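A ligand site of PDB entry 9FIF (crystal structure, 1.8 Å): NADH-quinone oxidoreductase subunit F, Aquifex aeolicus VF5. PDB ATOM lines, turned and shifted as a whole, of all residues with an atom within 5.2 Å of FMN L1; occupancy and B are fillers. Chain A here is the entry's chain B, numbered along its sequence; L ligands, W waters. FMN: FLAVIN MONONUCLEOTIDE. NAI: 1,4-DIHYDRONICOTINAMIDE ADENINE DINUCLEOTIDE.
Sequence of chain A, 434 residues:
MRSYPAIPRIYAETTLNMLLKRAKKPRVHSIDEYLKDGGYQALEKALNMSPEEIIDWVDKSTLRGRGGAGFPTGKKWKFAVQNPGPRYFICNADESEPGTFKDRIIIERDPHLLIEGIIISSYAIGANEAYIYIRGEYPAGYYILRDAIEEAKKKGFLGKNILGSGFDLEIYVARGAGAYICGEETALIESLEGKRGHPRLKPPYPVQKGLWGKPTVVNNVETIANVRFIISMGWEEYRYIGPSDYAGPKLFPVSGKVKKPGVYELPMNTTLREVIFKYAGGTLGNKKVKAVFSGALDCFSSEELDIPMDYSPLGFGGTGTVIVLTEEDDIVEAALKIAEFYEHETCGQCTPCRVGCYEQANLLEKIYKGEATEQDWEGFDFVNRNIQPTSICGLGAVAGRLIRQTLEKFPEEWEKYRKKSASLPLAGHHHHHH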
ATOM      1  N   GLY A  65      18.588 -20.558  -1.041  1.00  0.00           N
ATOM      2  CA  GLY A  65      17.248 -21.104  -0.902  1.00  0.00           C
ATOM      3  C   GLY A  65      17.211 -22.301   0.037  1.00  0.00           C
ATOM      4  O   GLY A  65      18.020 -23.220  -0.078  1.00  0.00           O
ATOM      5  N   ARG A  66      16.251 -22.303   0.968  1.00  0.00           N
ATOM      6  CA  ARG A  66      16.133 -23.365   1.951  1.00  0.00           C
ATOM      7  C   ARG A  66      15.051 -24.375   1.579  1.00  0.00           C
ATOM      8  O   ARG A  66      14.709 -25.240   2.371  1.00  0.00           O
ATOM      9  CB  ARG A  66      15.796 -22.770   3.323  1.00  0.00           C
ATOM     10  CG  ARG A  66      16.825 -21.791   3.850  1.00  0.00           C
ATOM     11  CD  ARG A  66      18.142 -22.419   4.232  1.00  0.00           C
ATOM     12  NE  ARG A  66      18.939 -21.483   5.017  1.00  0.00           N
ATOM     13  CZ  ARG A  66      20.134 -20.995   4.699  1.00  0.00           C
ATOM     14  NH1 ARG A  66      20.863 -20.425   5.641  1.00  0.00           N
ATOM     15  NH2 ARG A  66      20.630 -21.162   3.485  1.00  0.00           N
ATOM     16  N   GLY A  67      14.521 -24.263   0.353  1.00  0.00           N
ATOM     17  CA  GLY A  67      13.417 -25.113  -0.080  1.00  0.00           C
ATOM     18  C   GLY A  67      13.903 -26.329  -0.871  1.00  0.00           C
ATOM     19  O   GLY A  67      13.081 -27.098  -1.356  1.00  0.00           O
ATOM     20  N   GLY A  68      15.226 -26.478  -1.018  1.00  0.00           N
ATOM     21  CA  GLY A  68      15.753 -27.742  -1.520  1.00  0.00           C
ATOM     22  C   GLY A  68      16.754 -27.583  -2.648  1.00  0.00           C
ATOM     23  O   GLY A  68      17.611 -28.442  -2.827  1.00  0.00           O
ATOM     24  N   ALA A  69      16.636 -26.523  -3.447  1.00  0.00           N
ATOM     25  CA  ALA A  69      17.475 -26.376  -4.623  1.00  0.00           C
ATOM     26  C   ALA A  69      18.695 -25.480  -4.347  1.00  0.00           C
ATOM     27  O   ALA A  69      19.581 -25.399  -5.188  1.00  0.00           O
ATOM     28  CB  ALA A  69      16.655 -25.838  -5.757  1.00  0.00           C
ATOM     29  N   GLY A  70      18.690 -24.749  -3.222  1.00  0.00           N
ATOM     30  CA  GLY A  70      19.844 -23.980  -2.786  1.00  0.00           C
ATOM     31  C   GLY A  70      20.276 -22.893  -3.769  1.00  0.00           C
ATOM     32  O   GLY A  70      21.439 -22.543  -3.820  1.00  0.00           O
ATOM     33  N   PHE A  71      19.330 -22.296  -4.519  1.00  0.00           N
ATOM     34  CA  PHE A  71      19.666 -21.199  -5.398  1.00  0.00           C
ATOM     35  C   PHE A  71      19.979 -19.929  -4.593  1.00  0.00           C
ATOM     36  O   PHE A  71      19.289 -19.611  -3.622  1.00  0.00           O
ATOM     37  CB  PHE A  71      18.546 -20.944  -6.394  1.00  0.00           C
ATOM     38  CG  PHE A  71      19.037 -20.111  -7.557  1.00  0.00           C
ATOM     39  CD1 PHE A  71      18.989 -18.720  -7.504  1.00  0.00           C
ATOM     40  CD2 PHE A  71      19.586 -20.712  -8.687  1.00  0.00           C
ATOM     41  CE1 PHE A  71      19.459 -17.958  -8.555  1.00  0.00           C
ATOM     42  CE2 PHE A  71      20.054 -19.942  -9.742  1.00  0.00           C
ATOM     43  CZ  PHE A  71      19.991 -18.569  -9.674  1.00  0.00           C
ATOM     44  N   LYS A  76      18.630 -14.423  -7.261  1.00  0.00           N
ATOM     45  CA  LYS A  76      17.256 -14.630  -7.710  1.00  0.00           C
ATOM     46  C   LYS A  76      16.513 -13.289  -7.775  1.00  0.00           C
ATOM     47  O   LYS A  76      15.824 -12.997  -8.759  1.00  0.00           O
ATOM     48  CB  LYS A  76      16.492 -15.596  -6.817  1.00  0.00           C
ATOM     49  CG  LYS A  76      15.158 -16.025  -7.401  1.00  0.00           C
ATOM     50  CD  LYS A  76      14.279 -16.843  -6.465  1.00  0.00           C
ATOM     51  CE  LYS A  76      14.931 -18.068  -5.952  1.00  0.00           C
ATOM     52  NZ  LYS A  76      13.953 -18.958  -5.321  1.00  0.00           N
ATOM     53  N   ASN A  92       6.589 -19.680  -0.118  1.00  0.00           N
ATOM     54  CA  ASN A  92       6.256 -21.083  -0.284  1.00  0.00           C
ATOM     55  C   ASN A  92       6.193 -21.772   1.078  1.00  0.00           C
ATOM     56  O   ASN A  92       7.219 -22.106   1.649  1.00  0.00           O
ATOM     57  CB  ASN A  92       7.252 -21.759  -1.213  1.00  0.00           C
ATOM     58  CG  ASN A  92       6.830 -23.153  -1.630  1.00  0.00           C
ATOM     59  OD1 ASN A  92       5.990 -23.802  -0.994  1.00  0.00           O
ATOM     60  ND2 ASN A  92       7.408 -23.609  -2.727  1.00  0.00           N
ATOM     61  N   ASP A  94       4.361 -24.689   1.459  1.00  0.00           N
ATOM     62  CA  ASP A  94       3.682 -25.925   1.105  1.00  0.00           C
ATOM     63  C   ASP A  94       4.228 -27.137   1.854  1.00  0.00           C
ATOM     64  O   ASP A  94       3.548 -28.155   1.859  1.00  0.00           O
ATOM     65  CB  ASP A  94       3.684 -26.226  -0.382  1.00  0.00           C
ATOM     66  CG  ASP A  94       2.593 -27.202  -0.774  1.00  0.00           C
ATOM     67  OD1 ASP A  94       1.411 -26.820  -0.618  1.00  0.00           O
ATOM     68  OD2 ASP A  94       2.926 -28.370  -1.166  1.00  0.00           O
ATOM     69  N   GLU A  95       5.451 -27.047   2.394  1.00  0.00           N
ATOM     70  CA  GLU A  95       6.164 -28.078   3.155  1.00  0.00           C
ATOM     71  C   GLU A  95       5.403 -29.411   3.286  1.00  0.00           C
ATOM     72  O   GLU A  95       4.643 -29.611   4.232  1.00  0.00           O
ATOM     73  CB  GLU A  95       6.483 -27.507   4.531  1.00  0.00           C
ATOM     74  CG  GLU A  95       7.196 -28.494   5.471  1.00  0.00           C
ATOM     75  CD  GLU A  95       7.764 -27.827   6.696  1.00  0.00           C
ATOM     76  OE1 GLU A  95       6.976 -27.499   7.626  1.00  0.00           O
ATOM     77  OE2 GLU A  95       9.008 -27.621   6.729  1.00  0.00           O
ATOM     78  N   SER A  96       5.632 -30.332   2.323  1.00  0.00           N
ATOM     79  CA  SER A  96       4.943 -31.606   2.300  1.00  0.00           C
ATOM     80  C   SER A  96       5.874 -32.799   2.062  1.00  0.00           C
ATOM     81  O   SER A  96       5.422 -33.934   1.924  1.00  0.00           O
ATOM     82  CB  SER A  96       3.843 -31.590   1.271  1.00  0.00           C
ATOM     83  OG  SER A  96       2.802 -30.765   1.762  1.00  0.00           O
ATOM     84  N   ASP A 103       9.405 -25.643   8.602  1.00  0.00           N
ATOM     85  CA  ASP A 103       8.791 -24.370   8.256  1.00  0.00           C
ATOM     86  C   ASP A 103       7.595 -24.074   9.153  1.00  0.00           C
ATOM     87  O   ASP A 103       7.345 -22.904   9.510  1.00  0.00           O
ATOM     88  CB  ASP A 103       8.353 -24.305   6.805  1.00  0.00           C
ATOM     89  CG  ASP A 103       9.476 -24.427   5.791  1.00  0.00           C
ATOM     90  OD1 ASP A 103      10.641 -24.179   6.158  1.00  0.00           O
ATOM     91  OD2 ASP A 103       9.160 -24.757   4.624  1.00  0.00           O
ATOM     92  N   TYR A 180       1.367 -32.522  -2.969  1.00  0.00           N
ATOM     93  CA  TYR A 180       2.783 -32.246  -2.769  1.00  0.00           C
ATOM     94  C   TYR A 180       3.366 -31.425  -3.912  1.00  0.00           C
ATOM     95  O   TYR A 180       4.274 -30.621  -3.715  1.00  0.00           O
ATOM     96  CB  TYR A 180       3.551 -33.563  -2.653  1.00  0.00           C
ATOM     97  CG  TYR A 180       5.066 -33.448  -2.717  1.00  0.00           C
ATOM     98  CD1 TYR A 180       5.773 -32.782  -1.722  1.00  0.00           C
ATOM     99  CD2 TYR A 180       5.789 -34.054  -3.730  1.00  0.00           C
ATOM    100  CE1 TYR A 180       7.160 -32.688  -1.763  1.00  0.00           C
ATOM    101  CE2 TYR A 180       7.174 -33.965  -3.780  1.00  0.00           C
ATOM    102  CZ  TYR A 180       7.860 -33.306  -2.787  1.00  0.00           C
ATOM    103  OH  TYR A 180       9.208 -33.186  -2.847  1.00  0.00           O
ATOM    104  N   ILE A 181       2.859 -31.670  -5.132  1.00  0.00           N
ATOM    105  CA  ILE A 181       3.426 -31.038  -6.308  1.00  0.00           C
ATOM    106  C   ILE A 181       3.218 -29.529  -6.265  1.00  0.00           C
ATOM    107  O   ILE A 181       3.970 -28.803  -6.891  1.00  0.00           O
ATOM    108  CB  ILE A 181       2.874 -31.672  -7.607  1.00  0.00           C
ATOM    109  CG1 ILE A 181       3.679 -31.261  -8.823  1.00  0.00           C
ATOM    110  CG2 ILE A 181       1.387 -31.366  -7.811  1.00  0.00           C
ATOM    111  CD1 ILE A 181       5.156 -31.559  -8.683  1.00  0.00           C
ATOM    112  N   GLY A 183       4.092 -27.605  -4.091  1.00  0.00           N
ATOM    113  CA  GLY A 183       5.327 -27.007  -3.578  1.00  0.00           C
ATOM    114  C   GLY A 183       6.331 -26.638  -4.672  1.00  0.00           C
ATOM    115  O   GLY A 183       7.210 -25.795  -4.456  1.00  0.00           O
ATOM    116  N   GLU A 184       6.249 -27.312  -5.823  1.00  0.00           N
ATOM    117  CA  GLU A 184       7.045 -26.937  -6.976  1.00  0.00           C
ATOM    118  C   GLU A 184       6.565 -25.564  -7.434  1.00  0.00           C
ATOM    119  O   GLU A 184       5.369 -25.336  -7.601  1.00  0.00           O
ATOM    120  CB  GLU A 184       6.877 -27.990  -8.068  1.00  0.00           C
ATOM    121  CG  GLU A 184       7.965 -27.917  -9.138  1.00  0.00           C
ATOM    122  CD  GLU A 184       7.812 -26.916 -10.268  1.00  0.00           C
ATOM    123  OE1 GLU A 184       6.734 -26.345 -10.468  1.00  0.00           O
ATOM    124  OE2 GLU A 184       8.834 -26.713 -10.980  1.00  0.00           O
ATOM    125  N   GLU A 185       7.503 -24.625  -7.612  1.00  0.00           N
ATOM    126  CA  GLU A 185       7.158 -23.204  -7.660  1.00  0.00           C
ATOM    127  C   GLU A 185       6.212 -22.893  -8.822  1.00  0.00           C
ATOM    128  O   GLU A 185       5.317 -22.057  -8.667  1.00  0.00           O
ATOM    129  CB  GLU A 185       8.399 -22.334  -7.725  1.00  0.00           C
ATOM    130  CG  GLU A 185       9.257 -22.616  -8.958  1.00  0.00           C
ATOM    131  CD  GLU A 185      10.542 -21.821  -9.072  1.00  0.00           C
ATOM    132  OE1 GLU A 185      10.781 -20.945  -8.237  1.00  0.00           O
ATOM    133  OE2 GLU A 185      11.293 -22.131 -10.015  1.00  0.00           O
ATOM    134  N   VAL A 218       9.595 -16.634  -5.926  1.00  0.00           N
ATOM    135  CA  VAL A 218       9.159 -17.614  -4.962  1.00  0.00           C
ATOM    136  C   VAL A 218      10.334 -17.936  -4.047  1.00  0.00           C
ATOM    137  O   VAL A 218      11.421 -18.235  -4.549  1.00  0.00           O
ATOM    138  CB  VAL A 218       8.663 -18.899  -5.650  1.00  0.00           C
ATOM    139  CG1 VAL A 218       8.106 -19.899  -4.642  1.00  0.00           C
ATOM    140  CG2 VAL A 218       7.644 -18.577  -6.739  1.00  0.00           C
ATOM    141  N   ASN A 219      10.115 -17.815  -2.730  1.00  0.00           N
ATOM    142  CA  ASN A 219      11.086 -18.228  -1.715  1.00  0.00           C
ATOM    143  C   ASN A 219      10.399 -19.056  -0.639  1.00  0.00           C
ATOM    144  O   ASN A 219       9.243 -18.833  -0.277  1.00  0.00           O
ATOM    145  CB  ASN A 219      11.838 -17.059  -1.080  1.00  0.00           C
ATOM    146  CG  ASN A 219      13.032 -16.600  -1.879  1.00  0.00           C
ATOM    147  OD1 ASN A 219      13.967 -17.377  -2.155  1.00  0.00           O
ATOM    148  ND2 ASN A 219      13.029 -15.337  -2.255  1.00  0.00           N
ATOM    149  N   ASN A 220      11.182 -19.996  -0.101  1.00  0.00           N
ATOM    150  CA  ASN A 220      10.768 -20.842   1.002  1.00  0.00           C
ATOM    151  C   ASN A 220      10.645 -20.040   2.306  1.00  0.00           C
ATOM    152  O   ASN A 220      11.371 -19.078   2.533  1.00  0.00           O
ATOM    153  CB  ASN A 220      11.771 -21.968   1.117  1.00  0.00           C
ATOM    154  CG  ASN A 220      11.456 -22.867   2.289  1.00  0.00           C
ATOM    155  OD1 ASN A 220      10.537 -23.695   2.220  1.00  0.00           O
ATOM    156  ND2 ASN A 220      12.245 -22.730   3.336  1.00  0.00           N
ATOM    157  N   VAL A 221       9.725 -20.478   3.180  1.00  0.00           N
ATOM    158  CA  VAL A 221       9.508 -19.897   4.492  1.00  0.00           C
ATOM    159  C   VAL A 221      10.829 -19.662   5.218  1.00  0.00           C
ATOM    160  O   VAL A 221      11.085 -18.561   5.695  1.00  0.00           O
ATOM    161  CB  VAL A 221       8.592 -20.791   5.354  1.00  0.00           C
ATOM    162  CG1 VAL A 221       8.660 -20.461   6.840  1.00  0.00           C
ATOM    163  CG2 VAL A 221       7.150 -20.706   4.868  1.00  0.00           C
ATOM    164  N   THR A 223      13.925 -19.573   4.118  1.00  0.00           N
ATOM    165  CA  THR A 223      14.738 -18.575   3.422  1.00  0.00           C
ATOM    166  C   THR A 223      14.348 -17.173   3.897  1.00  0.00           C
ATOM    167  O   THR A 223      15.210 -16.356   4.220  1.00  0.00           O
ATOM    168  CB  THR A 223      14.586 -18.664   1.900  1.00  0.00           C
ATOM    169  OG1 THR A 223      14.768 -20.024   1.512  1.00  0.00           O
ATOM    170  CG2 THR A 223      15.581 -17.770   1.188  1.00  0.00           C
ATOM    171  N   CYS A 393       9.673 -31.426 -14.342  1.00  0.00           N
ATOM    172  CA  CYS A 393       9.953 -30.912 -13.004  1.00  0.00           C
ATOM    173  C   CYS A 393      10.814 -31.908 -12.231  1.00  0.00           C
ATOM    174  O   CYS A 393      11.064 -33.021 -12.673  1.00  0.00           O
ATOM    175  CB  CYS A 393       8.698 -30.505 -12.236  1.00  0.00           C
ATOM    176  SG  CYS A 393       7.906 -31.780 -11.210  1.00  0.00           S
ATOM    177  N   GLY A 394      11.256 -31.482 -11.037  1.00  0.00           N
ATOM    178  CA  GLY A 394      12.196 -32.241 -10.218  1.00  0.00           C
ATOM    179  C   GLY A 394      11.640 -33.546  -9.659  1.00  0.00           C
ATOM    180  O   GLY A 394      12.429 -34.422  -9.321  1.00  0.00           O
ATOM    181  N   LEU A 395      10.294 -33.710  -9.571  1.00  0.00           N
ATOM    182  CA  LEU A 395       9.713 -34.903  -8.993  1.00  0.00           C
ATOM    183  C   LEU A 395      10.113 -36.117  -9.823  1.00  0.00           C
ATOM    184  O   LEU A 395      10.583 -37.122  -9.296  1.00  0.00           O
ATOM    185  CB  LEU A 395       8.188 -34.801  -8.835  1.00  0.00           C
ATOM    186  CG  LEU A 395       7.522 -35.905  -8.000  1.00  0.00           C
ATOM    187  CD1 LEU A 395       6.271 -35.430  -7.302  1.00  0.00           C
ATOM    188  CD2 LEU A 395       7.200 -37.154  -8.828  1.00  0.00           C
HETATM  189  N1  FMN L   1       9.982 -25.463  -1.988  1.00  0.00           N
HETATM  190  C2  FMN L   1       9.434 -24.995  -0.822  1.00  0.00           C
HETATM  191  O2  FMN L   1       9.724 -23.887  -0.369  1.00  0.00           O
HETATM  192  N3  FMN L   1       8.487 -25.793  -0.233  1.00  0.00           N
HETATM  193  C4  FMN L   1       8.019 -27.012  -0.714  1.00  0.00           C
HETATM  194  O4  FMN L   1       7.141 -27.602  -0.082  1.00  0.00           O
HETATM  195  C4A FMN L   1       8.623 -27.426  -1.954  1.00  0.00           C
HETATM  196  N5  FMN L   1       8.184 -28.564  -2.556  1.00  0.00           N
HETATM  197  C5A FMN L   1       8.682 -28.936  -3.820  1.00  0.00           C
HETATM  198  C6  FMN L   1       8.190 -30.073  -4.458  1.00  0.00           C
HETATM  199  C7  FMN L   1       8.688 -30.466  -5.696  1.00  0.00           C
HETATM  200  C7M FMN L   1       8.144 -31.714  -6.358  1.00  0.00           C
HETATM  201  C8  FMN L   1       9.706 -29.706  -6.303  1.00  0.00           C
HETATM  202  C8M FMN L   1      10.353 -30.154  -7.581  1.00  0.00           C
HETATM  203  C9  FMN L   1      10.186 -28.562  -5.668  1.00  0.00           C
HETATM  204  C9A FMN L   1       9.686 -28.174  -4.437  1.00  0.00           C
HETATM  205  N10 FMN L   1      10.164 -27.000  -3.771  1.00  0.00           N
HETATM  206  C10 FMN L   1       9.598 -26.652  -2.559  1.00  0.00           C
HETATM  207  C1' FMN L   1      11.189 -26.155  -4.398  1.00  0.00           C
HETATM  208  C2' FMN L   1      10.535 -24.951  -5.091  1.00  0.00           C
HETATM  209  O2' FMN L   1      10.168 -25.298  -6.428  1.00  0.00           O
HETATM  210  C3' FMN L   1      11.480 -23.753  -5.109  1.00  0.00           C
HETATM  211  O3' FMN L   1      12.805 -24.083  -5.530  1.00  0.00           O
HETATM  212  C4' FMN L   1      11.573 -22.967  -3.789  1.00  0.00           C
HETATM  213  O4' FMN L   1      10.299 -22.709  -3.189  1.00  0.00           O
HETATM  214  C5' FMN L   1      12.328 -21.681  -4.022  1.00  0.00           C
HETATM  215  O5' FMN L   1      12.551 -20.964  -2.777  1.00  0.00           O
HETATM  216  P   FMN L   1      14.038 -20.985  -2.160  1.00  0.00           P
HETATM  217  O1P FMN L   1      14.962 -20.461  -3.236  1.00  0.00           O
HETATM  218  O2P FMN L   1      13.886 -20.036  -0.980  1.00  0.00           O
HETATM  219  O3P FMN L   1      14.340 -22.408  -1.747  1.00  0.00           O
HETATM  220  PA  NAI L   2      15.597 -25.493  -9.152  1.00  0.00           P
HETATM  221  O1A NAI L   2      17.011 -25.925  -9.153  1.00  0.00           O
HETATM  222  O2A NAI L   2      14.950 -25.494 -10.519  1.00  0.00           O
HETATM  223  O5B NAI L   2      15.210 -24.049  -8.523  1.00  0.00           O
HETATM  224  C5B NAI L   2      16.017 -23.210  -7.665  1.00  0.00           C
HETATM  225  C4B NAI L   2      15.365 -21.871  -7.508  1.00  0.00           C
HETATM  226  O4B NAI L   2      16.169 -20.908  -8.239  1.00  0.00           O
HETATM  227  C3B NAI L   2      13.966 -21.715  -8.075  1.00  0.00           C
HETATM  228  O3B NAI L   2      13.287 -20.618  -7.463  1.00  0.00           O
HETATM  229  C2B NAI L   2      14.247 -21.385  -9.542  1.00  0.00           C
HETATM  230  O2B NAI L   2      13.231 -20.602 -10.162  1.00  0.00           O
HETATM  231  C1B NAI L   2      15.487 -20.478  -9.399  1.00  0.00           C
HETATM  232  N9A NAI L   2      16.410 -20.530 -10.529  1.00  0.00           N
HETATM  233  C8A NAI L   2      17.219 -21.566 -10.910  1.00  0.00           C
HETATM  234  N7A NAI L   2      17.975 -21.306 -11.955  1.00  0.00           N
HETATM  235  C5A NAI L   2      17.638 -19.993 -12.276  1.00  0.00           C
HETATM  236  C6A NAI L   2      18.094 -19.121 -13.273  1.00  0.00           C
HETATM  237  N6A NAI L   2      19.039 -19.434 -14.167  1.00  0.00           N
HETATM  238  N1A NAI L   2      17.553 -17.884 -13.323  1.00  0.00           N
HETATM  239  C2A NAI L   2      16.633 -17.553 -12.410  1.00  0.00           C
HETATM  240  N3A NAI L   2      16.133 -18.286 -11.418  1.00  0.00           N
HETATM  241  C4A NAI L   2      16.671 -19.508 -11.402  1.00  0.00           C
HETATM  242  O3  NAI L   2      14.768 -26.480  -8.204  1.00  0.00           O
HETATM  243  PN  NAI L   2      13.276 -27.005  -8.041  1.00  0.00           P
HETATM  244  O1N NAI L   2      13.066 -28.038  -9.159  1.00  0.00           O
HETATM  245  O2N NAI L   2      12.255 -25.961  -8.000  1.00  0.00           O
HETATM  246  O5D NAI L   2      13.443 -27.770  -6.568  1.00  0.00           O
HETATM  247  C5D NAI L   2      13.982 -29.044  -6.129  1.00  0.00           C
HETATM  248  C4D NAI L   2      13.841 -29.136  -4.621  1.00  0.00           C
HETATM  249  O   HOH W   1      11.089 -28.824  -0.459  1.00  0.00           O
HETATM  250  O   HOH W   2      16.830 -18.499  -2.950  1.00  0.00           O
HETATM  251  O   HOH W   3       8.260 -30.027   0.827  1.00  0.00           O
HETATM  252  O   HOH W   4       7.506 -24.779   2.386  1.00  0.00           O
HETATM  253  O   HOH W   5      14.731 -24.413  -3.391  1.00  0.00           O
HETATM  254  O   HOH W   6       5.314 -29.506  -1.232  1.00  0.00           O
HETATM  255  O   HOH W   7      10.030 -30.971  -1.334  1.00  0.00           O
HETATM  256  O   HOH W   8      16.498 -22.333  -4.373  1.00  0.00           O
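O of Gly 183 lies close to N10 of FMN L1.
The backbone carbonyl oxygen (O) of Val 218 sits close to an oxygen (O5') of FMN L1 (3.4 Å).
Merely in contact with FMN L1: Gly 65 (3.3 Å), Asp 94 (3.5 Å), Glu 184 (3.5 Å), Tyr 180 (3.6 Å), Ile 181 (3.8 Å), Gly 394 (3.8 Å), Ser 96 (3.9 Å) and Leu 395 (3.96 Å).
Hydrophobic or aromatic side chains within 4 Å of FMN L1: Tyr 180, Ile 181, Val 218 and Leu 395.
Within 4 Å of FMN L1: Gly 65, Arg 66, Gly 67, Lys 76, Asn 92, Asp 94, Glu 95, Ser 96, Tyr 180, Ile 181, Gly 183, Glu 184, Glu 185, Val 218, Asn 219, Asn 220, Thr 223, Gly 394 and Leu 395.
Along chain A the residues within 4 Å of FMN L1 span positions 65 to 395.
The nearest printed residue that does not touch FMN L1 is Gly 68 (4.2 Å).
The backbone NH (N) of Asn 92 lies within hydrogen-bond range of the backbone carbonyl oxygen (O) of Asn 219 (2.8 Å).
The side-chain amide nitrogen of Asn 92 is in hydrogen-bond range of the backbone carbonyl oxygen of Gly 183 (2.8 Å).
O of Asp 94 is in hydrogen-bond range of OG of Ser 96, at 2.7 Å.
The backbone carbonyl oxygen (O) of Phe 71 sits at hydrogen-bond distance from the backbone NH (N) of Gly 65, at 2.8 Å.
N of Gly 183 is in hydrogen-bond range of OD2 of Asp 94 (3.2 Å).
The side-chain amino group (NZ) of Lys 76 lies within hydrogen-bond range of the backbone carbonyl oxygen (O) of Val 218.
The side-chain hydroxyl (OG1) of Thr 223 sits at hydrogen-bond distance from the backbone NH (N) of Arg 66.
The backbone NH of Asp 103 sits at hydrogen-bond distance from the side-chain carboxylate of Glu 95 (2.8 Å).
Water W5 lies within hydrogen-bond range of an oxygen (O3P) of FMN L1 (2.6 Å), the backbone NH of Ala 69 (2.8 Å) and the backbone NH of Gly 68 (3.2 Å).
Water W8 lies within hydrogen-bond range of an oxygen (O1P) of FMN L1, the backbone NH (N) of Phe 71 and the backbone NH (N) of Gly 70.
Water W2 lies within hydrogen-bond range of O1P of FMN L1 (2.7 Å), O of Phe 71 (2.8 Å), OD1 of Asn 219 (3.2 Å) and N of Gly 65 (3.3 Å).
Water W3 bridges O4 of FMN L1 (2.8 Å) and N of Ser 96 (3.0 Å).
Water W7 bridges the side-chain hydroxyl (OH) of Tyr 180 (2.8 Å) and a nitrogen (N5) of FMN L1 (3.3 Å).
O2' of FMN L1 lies within hydrogen-bond range of N of Glu 185, 3.0 Å away.
O2 of FMN L1 sits close to OD1 of Asn 220 (2.7 Å).
O4' of FMN L1 is in hydrogen-bond range of ND2 of Asn 92 (3.1 Å).
The backbone NH of Asn 220 lies within hydrogen-bond range of an oxygen (O2P) of FMN L1.
OE2 of Glu 185 is in hydrogen-bond range of O2B of NAI L2 (2.5 Å).
An oxygen (O3B) of NAI L2 sits at hydrogen-bond distance from the side-chain amino group (NZ) of Lys 76 (2.8 Å).
OD1 of Asn 219 sits close to O2P of FMN L1.
O3P of FMN L1 sits at hydrogen-bond distance from N of Gly 67 (2.8 Å).
An oxygen (O1P) of FMN L1 lies within salt-bridge range of the side-chain amino group (NZ) of Lys 76 (2.8 Å).
OG1 of Thr 223 is in hydrogen-bond range of O2P of FMN L1 (2.6 Å).
An oxygen (O3P) of FMN L1 sits at hydrogen-bond distance from the backbone NH of Arg 66.
An oxygen (O4) of FMN L1 sits at hydrogen-bond distance from the backbone NH (N) of Glu 95, 3.0 Å away.
An oxygen (O2') of FMN L1 sits at hydrogen-bond distance from an oxygen (O2N) of NAI L2 (2.7 Å).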
